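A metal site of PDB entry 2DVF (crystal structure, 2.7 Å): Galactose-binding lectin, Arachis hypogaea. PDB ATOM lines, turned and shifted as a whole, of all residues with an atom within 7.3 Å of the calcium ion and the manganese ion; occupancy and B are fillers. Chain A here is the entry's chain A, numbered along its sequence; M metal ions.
The calcium ion is bound by O of Tyr 125, OD1 of Asp 123, OD2 of Asp 132, OD1 of Asn 127 and OD2 of Asp 123.
Residues that only touch the calcium ion: Gly 104 (3.8 Å) and Asp 83 (3.96 Å).
Six residues have an atom within 4 Å of the calcium ion: Asp 83, Gly 104, Asp 123, Tyr 125, Asn 127 and Asp 132.
The nearest printed residue that does not touch the calcium ion is Ser 126 (4.7 Å).
The manganese ion is bound by OE2 of Glu 121, 2.1 Å away.
The manganese ion is bound by OD1 of Asp 132.
The manganese ion is bound by NE2 of His 137 (2.4 Å).
The manganese ion is bound by OD2 of Asp 123 (2.5 Å).
The manganese ion has four donor atoms within binding distance.
Residues that only touch the manganese ion: Val 145 and Ser 147.
Of the 28 residues printed, 6 come within 4 Å of the manganese ion.
OE1 of Glu 121 sits close to OD2 of Asp 141 (2.7 Å).
The backbone NH of Gly 104 sits at hydrogen-bond distance from the side-chain carboxylate of Asp 83 (3.3 Å).
The backbone NH (N) of Glu 121 lies within hydrogen-bond range of the backbone carbonyl oxygen (O) of Gly 139.
The side-chain hydroxyl (OG) of Ser 147 sits at hydrogen-bond distance from the side-chain carboxylate (OD1) of Asp 141.
The side-chain hydroxyl of Thr 124 sits at hydrogen-bond distance from the backbone carbonyl oxygen of Asp 83, at 3.3 Å.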
ATOM      1  N   ALA A  82      -0.419   2.074  11.462  1.00  0.00           N
ATOM      2  CA  ALA A  82       0.242   3.346  11.654  1.00  0.00           C
ATOM      3  C   ALA A  82       1.415   3.085  12.590  1.00  0.00           C
ATOM      4  O   ALA A  82       1.442   2.043  13.259  1.00  0.00           O
ATOM      5  CB  ALA A  82      -0.722   4.343  12.267  1.00  0.00           C
ATOM      6  N   ASP A  83       2.370   4.006  12.663  1.00  0.00           N
ATOM      7  CA  ASP A  83       2.331   5.258  11.906  1.00  0.00           C
ATOM      8  C   ASP A  83       3.336   5.336  10.754  1.00  0.00           C
ATOM      9  O   ASP A  83       3.150   6.113   9.818  1.00  0.00           O
ATOM     10  CB  ASP A  83       2.552   6.432  12.870  1.00  0.00           C
ATOM     11  CG  ASP A  83       1.263   7.118  13.243  1.00  0.00           C
ATOM     12  OD1 ASP A  83       0.861   8.049  12.502  1.00  0.00           O
ATOM     13  OD2 ASP A  83       0.641   6.753  14.260  1.00  0.00           O
ATOM     14  N   GLY A  84       4.397   4.542  10.831  1.00  0.00           N
ATOM     15  CA  GLY A  84       5.391   4.564   9.774  1.00  0.00           C
ATOM     16  C   GLY A  84       6.833   4.430  10.214  1.00  0.00           C
ATOM     17  O   GLY A  84       7.130   4.313  11.397  1.00  0.00           O
ATOM     18  N   GLY A 103       2.718   8.764  17.174  1.00  0.00           N
ATOM     19  CA  GLY A 103       1.891   9.026  16.017  1.00  0.00           C
ATOM     20  C   GLY A 103       2.582   9.577  14.777  1.00  0.00           C
ATOM     21  O   GLY A 103       3.607   9.058  14.335  1.00  0.00           O
ATOM     22  N   GLY A 104       1.991  10.623  14.215  1.00  0.00           N
ATOM     23  CA  GLY A 104       2.532  11.238  13.016  1.00  0.00           C
ATOM     24  C   GLY A 104       3.849  11.977  13.182  1.00  0.00           C
ATOM     25  O   GLY A 104       4.319  12.603  12.230  1.00  0.00           O
ATOM     26  N   THR A 105       4.456  11.935  14.360  1.00  0.00           N
ATOM     27  CA  THR A 105       5.724  12.630  14.560  1.00  0.00           C
ATOM     28  C   THR A 105       6.870  11.699  14.170  1.00  0.00           C
ATOM     29  O   THR A 105       8.009  12.138  14.027  1.00  0.00           O
ATOM     30  CB  THR A 105       5.921  13.044  16.023  1.00  0.00           C
ATOM     31  OG1 THR A 105       6.340  11.896  16.791  1.00  0.00           O
ATOM     32  CG2 THR A 105       4.615  13.586  16.597  1.00  0.00           C
ATOM     33  N   LEU A 106       6.540  10.425  14.014  1.00  0.00           N
ATOM     34  CA  LEU A 106       7.473   9.373  13.642  1.00  0.00           C
ATOM     35  C   LEU A 106       8.642   9.232  14.598  1.00  0.00           C
ATOM     36  O   LEU A 106       9.644   8.588  14.285  1.00  0.00           O
ATOM     37  CB  LEU A 106       7.975   9.607  12.216  1.00  0.00           C
ATOM     38  CG  LEU A 106       6.879   9.761  11.165  1.00  0.00           C
ATOM     39  CD1 LEU A 106       7.505   9.810   9.773  1.00  0.00           C
ATOM     40  CD2 LEU A 106       5.878   8.609  11.258  1.00  0.00           C
ATOM     41  N   GLU A 121      10.701   9.580   4.975  1.00  0.00           N
ATOM     42  CA  GLU A 121       9.665   8.884   5.699  1.00  0.00           C
ATOM     43  C   GLU A 121       8.848   7.922   4.828  1.00  0.00           C
ATOM     44  O   GLU A 121       8.775   8.062   3.610  1.00  0.00           O
ATOM     45  CB  GLU A 121       8.738   9.877   6.391  1.00  0.00           C
ATOM     46  CG  GLU A 121       8.041  10.835   5.459  1.00  0.00           C
ATOM     47  CD  GLU A 121       6.860  11.489   6.118  1.00  0.00           C
ATOM     48  OE1 GLU A 121       7.056  12.237   7.086  1.00  0.00           O
ATOM     49  OE2 GLU A 121       5.724  11.244   5.668  1.00  0.00           O
ATOM     50  N   PHE A 122       8.266   6.943   5.507  1.00  0.00           N
ATOM     51  CA  PHE A 122       7.433   5.927   4.879  1.00  0.00           C
ATOM     52  C   PHE A 122       6.163   5.961   5.704  1.00  0.00           C
ATOM     53  O   PHE A 122       5.884   5.093   6.544  1.00  0.00           O
ATOM     54  CB  PHE A 122       8.154   4.586   4.939  1.00  0.00           C
ATOM     55  CG  PHE A 122       9.460   4.580   4.202  1.00  0.00           C
ATOM     56  CD1 PHE A 122       9.494   4.404   2.817  1.00  0.00           C
ATOM     57  CD2 PHE A 122      10.655   4.834   4.877  1.00  0.00           C
ATOM     58  CE1 PHE A 122      10.707   4.460   2.126  1.00  0.00           C
ATOM     59  CE2 PHE A 122      11.861   4.900   4.192  1.00  0.00           C
ATOM     60  CZ  PHE A 122      11.894   4.711   2.813  1.00  0.00           C
ATOM     61  N   ASP A 123       5.420   7.018   5.436  1.00  0.00           N
ATOM     62  CA  ASP A 123       4.176   7.354   6.100  1.00  0.00           C
ATOM     63  C   ASP A 123       2.989   6.471   5.687  1.00  0.00           C
ATOM     64  O   ASP A 123       2.625   6.399   4.513  1.00  0.00           O
ATOM     65  CB  ASP A 123       3.884   8.819   5.823  1.00  0.00           C
ATOM     66  CG  ASP A 123       3.114   9.488   6.922  1.00  0.00           C
ATOM     67  OD1 ASP A 123       2.201   8.832   7.469  1.00  0.00           O
ATOM     68  OD2 ASP A 123       3.406  10.662   7.229  1.00  0.00           O
ATOM     69  N   THR A 124       2.387   5.821   6.670  1.00  0.00           N
ATOM     70  CA  THR A 124       1.263   4.926   6.425  1.00  0.00           C
ATOM     71  C   THR A 124      -0.027   5.447   7.050  1.00  0.00           C
ATOM     72  O   THR A 124      -1.027   4.725   7.104  1.00  0.00           O
ATOM     73  CB  THR A 124       1.532   3.556   7.008  1.00  0.00           C
ATOM     74  OG1 THR A 124       1.555   3.643   8.428  1.00  0.00           O
ATOM     75  CG2 THR A 124       2.880   3.023   6.530  1.00  0.00           C
ATOM     76  N   TYR A 125       0.002   6.673   7.555  1.00  0.00           N
ATOM     77  CA  TYR A 125      -1.183   7.266   8.151  1.00  0.00           C
ATOM     78  C   TYR A 125      -1.291   8.747   7.806  1.00  0.00           C
ATOM     79  O   TYR A 125      -0.390   9.528   8.108  1.00  0.00           O
ATOM     80  CB  TYR A 125      -1.159   7.067   9.676  1.00  0.00           C
ATOM     81  CG  TYR A 125      -2.437   7.498  10.366  1.00  0.00           C
ATOM     82  CD1 TYR A 125      -2.660   8.833  10.707  1.00  0.00           C
ATOM     83  CD2 TYR A 125      -3.438   6.574  10.653  1.00  0.00           C
ATOM     84  CE1 TYR A 125      -3.846   9.243  11.315  1.00  0.00           C
ATOM     85  CE2 TYR A 125      -4.633   6.967  11.278  1.00  0.00           C
ATOM     86  CZ  TYR A 125      -4.826   8.295  11.602  1.00  0.00           C
ATOM     87  OH  TYR A 125      -5.991   8.694  12.205  1.00  0.00           O
ATOM     88  N   SER A 126      -2.385   9.139   7.169  1.00  0.00           N
ATOM     89  CA  SER A 126      -2.563  10.533   6.777  1.00  0.00           C
ATOM     90  C   SER A 126      -2.921  11.481   7.920  1.00  0.00           C
ATOM     91  O   SER A 126      -4.053  11.518   8.381  1.00  0.00           O
ATOM     92  CB  SER A 126      -3.630  10.625   5.686  1.00  0.00           C
ATOM     93  OG  SER A 126      -3.816  11.958   5.272  1.00  0.00           O
ATOM     94  N   ASN A 127      -1.932  12.263   8.367  1.00  0.00           N
ATOM     95  CA  ASN A 127      -2.105  13.240   9.439  1.00  0.00           C
ATOM     96  C   ASN A 127      -2.293  14.609   8.809  1.00  0.00           C
ATOM     97  O   ASN A 127      -1.333  15.221   8.356  1.00  0.00           O
ATOM     98  CB  ASN A 127      -0.882  13.291  10.350  1.00  0.00           C
ATOM     99  CG  ASN A 127      -0.774  12.090  11.243  1.00  0.00           C
ATOM    100  OD1 ASN A 127      -0.560  10.985  10.787  1.00  0.00           O
ATOM    101  ND2 ASN A 127      -0.935  12.298  12.543  1.00  0.00           N
ATOM    102  N   SER A 128      -3.529  15.112   8.805  1.00  0.00           N
ATOM    103  CA  SER A 128      -3.815  16.421   8.222  1.00  0.00           C
ATOM    104  C   SER A 128      -3.115  17.547   8.961  1.00  0.00           C
ATOM    105  O   SER A 128      -2.829  18.590   8.377  1.00  0.00           O
ATOM    106  CB  SER A 128      -5.325  16.665   8.218  1.00  0.00           C
ATOM    107  OG  SER A 128      -5.843  16.670   9.534  1.00  0.00           O
ATOM    108  N   TYR A 130      -0.278  17.646   9.724  1.00  0.00           N
ATOM    109  CA  TYR A 130       1.084  17.713   9.199  1.00  0.00           C
ATOM    110  C   TYR A 130       0.976  17.779   7.685  1.00  0.00           C
ATOM    111  O   TYR A 130       1.962  17.624   6.969  1.00  0.00           O
ATOM    112  CB  TYR A 130       1.892  16.477   9.611  1.00  0.00           C
ATOM    113  CG  TYR A 130       1.952  16.243  11.109  1.00  0.00           C
ATOM    114  CD1 TYR A 130       2.323  17.263  11.990  1.00  0.00           C
ATOM    115  CD2 TYR A 130       1.663  14.986  11.642  1.00  0.00           C
ATOM    116  CE1 TYR A 130       2.402  17.033  13.359  1.00  0.00           C
ATOM    117  CE2 TYR A 130       1.733  14.751  13.013  1.00  0.00           C
ATOM    118  CZ  TYR A 130       2.107  15.774  13.861  1.00  0.00           C
ATOM    119  OH  TYR A 130       2.172  15.542  15.220  1.00  0.00           O
ATOM    120  N   ASN A 131      -0.246  17.991   7.211  1.00  0.00           N
ATOM    121  CA  ASN A 131      -0.531  18.085   5.780  1.00  0.00           C
ATOM    122  C   ASN A 131      -0.184  16.816   5.020  1.00  0.00           C
ATOM    123  O   ASN A 131       0.265  16.881   3.887  1.00  0.00           O
ATOM    124  CB  ASN A 131       0.224  19.275   5.177  1.00  0.00           C
ATOM    125  CG  ASN A 131      -0.310  20.594   5.661  1.00  0.00           C
ATOM    126  OD1 ASN A 131      -1.457  20.961   5.381  1.00  0.00           O
ATOM    127  ND2 ASN A 131       0.517  21.335   6.399  1.00  0.00           N
ATOM    128  N   ASP A 132      -0.391  15.660   5.639  1.00  0.00           N
ATOM    129  CA  ASP A 132      -0.095  14.400   4.978  1.00  0.00           C
ATOM    130  C   ASP A 132      -0.932  14.221   3.725  1.00  0.00           C
ATOM    131  O   ASP A 132      -2.073  14.672   3.661  1.00  0.00           O
ATOM    132  CB  ASP A 132      -0.361  13.195   5.910  1.00  0.00           C
ATOM    133  CG  ASP A 132       0.852  12.788   6.721  1.00  0.00           C
ATOM    134  OD1 ASP A 132       1.988  13.052   6.279  1.00  0.00           O
ATOM    135  OD2 ASP A 132       0.672  12.181   7.783  1.00  0.00           O
ATOM    136  N   PRO A 133      -0.373  13.571   2.700  1.00  0.00           N
ATOM    137  CA  PRO A 133      -1.121  13.356   1.467  1.00  0.00           C
ATOM    138  C   PRO A 133      -2.278  12.419   1.833  1.00  0.00           C
ATOM    139  O   PRO A 133      -2.268  11.787   2.885  1.00  0.00           O
ATOM    140  CB  PRO A 133      -0.112  12.678   0.559  1.00  0.00           C
ATOM    141  CG  PRO A 133       1.202  13.196   1.050  1.00  0.00           C
ATOM    142  CD  PRO A 133       1.036  13.148   2.539  1.00  0.00           C
ATOM    143  N   HIS A 137       2.549   7.334   1.565  1.00  0.00           N
ATOM    144  CA  HIS A 137       3.533   8.083   0.807  1.00  0.00           C
ATOM    145  C   HIS A 137       4.970   7.989   1.317  1.00  0.00           C
ATOM    146  O   HIS A 137       5.232   7.640   2.476  1.00  0.00           O
ATOM    147  CB  HIS A 137       3.127   9.551   0.788  1.00  0.00           C
ATOM    148  CG  HIS A 137       2.940  10.123   2.155  1.00  0.00           C
ATOM    149  ND1 HIS A 137       1.827   9.860   2.918  1.00  0.00           N
ATOM    150  CD2 HIS A 137       3.739  10.918   2.914  1.00  0.00           C
ATOM    151  CE1 HIS A 137       1.948  10.456   4.097  1.00  0.00           C
ATOM    152  NE2 HIS A 137       3.104  11.108   4.112  1.00  0.00           N
ATOM    153  N   VAL A 138       5.905   8.318   0.432  1.00  0.00           N
ATOM    154  CA  VAL A 138       7.321   8.354   0.754  1.00  0.00           C
ATOM    155  C   VAL A 138       7.618   9.860   0.750  1.00  0.00           C
ATOM    156  O   VAL A 138       7.142  10.569  -0.140  1.00  0.00           O
ATOM    157  CB  VAL A 138       8.188   7.655  -0.326  1.00  0.00           C
ATOM    158  CG1 VAL A 138       9.655   7.762   0.016  1.00  0.00           C
ATOM    159  CG2 VAL A 138       7.797   6.196  -0.441  1.00  0.00           C
ATOM    160  N   GLY A 139       8.356  10.348   1.734  1.00  0.00           N
ATOM    161  CA  GLY A 139       8.626  11.768   1.758  1.00  0.00           C
ATOM    162  C   GLY A 139       9.987  12.197   2.243  1.00  0.00           C
ATOM    163  O   GLY A 139      10.646  11.487   2.996  1.00  0.00           O
ATOM    164  N   ASP A 141      11.876  14.756   4.463  1.00  0.00           N
ATOM    165  CA  ASP A 141      11.613  15.661   5.566  1.00  0.00           C
ATOM    166  C   ASP A 141      12.830  16.496   5.935  1.00  0.00           C
ATOM    167  O   ASP A 141      13.959  15.998   5.951  1.00  0.00           O
ATOM    168  CB  ASP A 141      11.127  14.877   6.787  1.00  0.00           C
ATOM    169  CG  ASP A 141       9.831  14.119   6.534  1.00  0.00           C
ATOM    170  OD1 ASP A 141       9.044  14.554   5.658  1.00  0.00           O
ATOM    171  OD2 ASP A 141       9.596  13.105   7.207  1.00  0.00           O
ATOM    172  N   SER A 144      10.900  18.640   9.816  1.00  0.00           N
ATOM    173  CA  SER A 144       9.457  18.598   9.974  1.00  0.00           C
ATOM    174  C   SER A 144       8.815  17.383   9.336  1.00  0.00           C
ATOM    175  O   SER A 144       9.258  16.939   8.271  1.00  0.00           O
ATOM    176  CB  SER A 144       8.815  19.852   9.375  1.00  0.00           C
ATOM    177  OG  SER A 144       7.411  19.690   9.271  1.00  0.00           O
ATOM    178  N   VAL A 145       7.785  16.829   9.977  1.00  0.00           N
ATOM    179  CA  VAL A 145       7.091  15.681   9.407  1.00  0.00           C
ATOM    180  C   VAL A 145       6.093  16.198   8.380  1.00  0.00           C
ATOM    181  O   VAL A 145       5.306  15.434   7.834  1.00  0.00           O
ATOM    182  CB  VAL A 145       6.347  14.824  10.456  1.00  0.00           C
ATOM    183  CG1 VAL A 145       7.332  13.966  11.223  1.00  0.00           C
ATOM    184  CG2 VAL A 145       5.529  15.704  11.378  1.00  0.00           C
ATOM    185  N   ASP A 146       6.131  17.506   8.151  1.00  0.00           N
ATOM    186  CA  ASP A 146       5.301  18.106   7.116  1.00  0.00           C
ATOM    187  C   ASP A 146       6.314  18.084   5.980  1.00  0.00           C
ATOM    188  O   ASP A 146       7.054  19.039   5.770  1.00  0.00           O
ATOM    189  CB  ASP A 146       4.947  19.550   7.461  1.00  0.00           C
ATOM    190  CG  ASP A 146       4.057  20.195   6.394  1.00  0.00           C
ATOM    191  OD1 ASP A 146       4.295  19.985   5.186  1.00  0.00           O
ATOM    192  OD2 ASP A 146       3.119  20.937   6.761  1.00  0.00           O
ATOM    193  N   SER A 147       6.359  16.977   5.256  1.00  0.00           N
ATOM    194  CA  SER A 147       7.311  16.791   4.176  1.00  0.00           C
ATOM    195  C   SER A 147       7.459  17.964   3.194  1.00  0.00           C
ATOM    196  O   SER A 147       6.519  18.699   2.912  1.00  0.00           O
ATOM    197  CB  SER A 147       6.956  15.514   3.400  1.00  0.00           C
ATOM    198  OG  SER A 147       6.720  14.437   4.298  1.00  0.00           O
ATOM    199  N   THR A 150       6.514  14.813  -1.198  1.00  0.00           N
ATOM    200  CA  THR A 150       6.031  13.453  -0.950  1.00  0.00           C
ATOM    201  C   THR A 150       5.780  12.806  -2.300  1.00  0.00           C
ATOM    202  O   THR A 150       5.748  13.485  -3.329  1.00  0.00           O
ATOM    203  CB  THR A 150       4.717  13.446  -0.124  1.00  0.00           C
ATOM    204  OG1 THR A 150       3.671  14.116  -0.858  1.00  0.00           O
ATOM    205  CG2 THR A 150       4.909  14.156   1.199  1.00  0.00           C
HETATM  206 CA    CA M   1       1.617  10.375   9.383  1.00  0.00          CA
HETATM  207 MN    MN M   2       4.057  12.575   5.789  1.00  0.00          MN
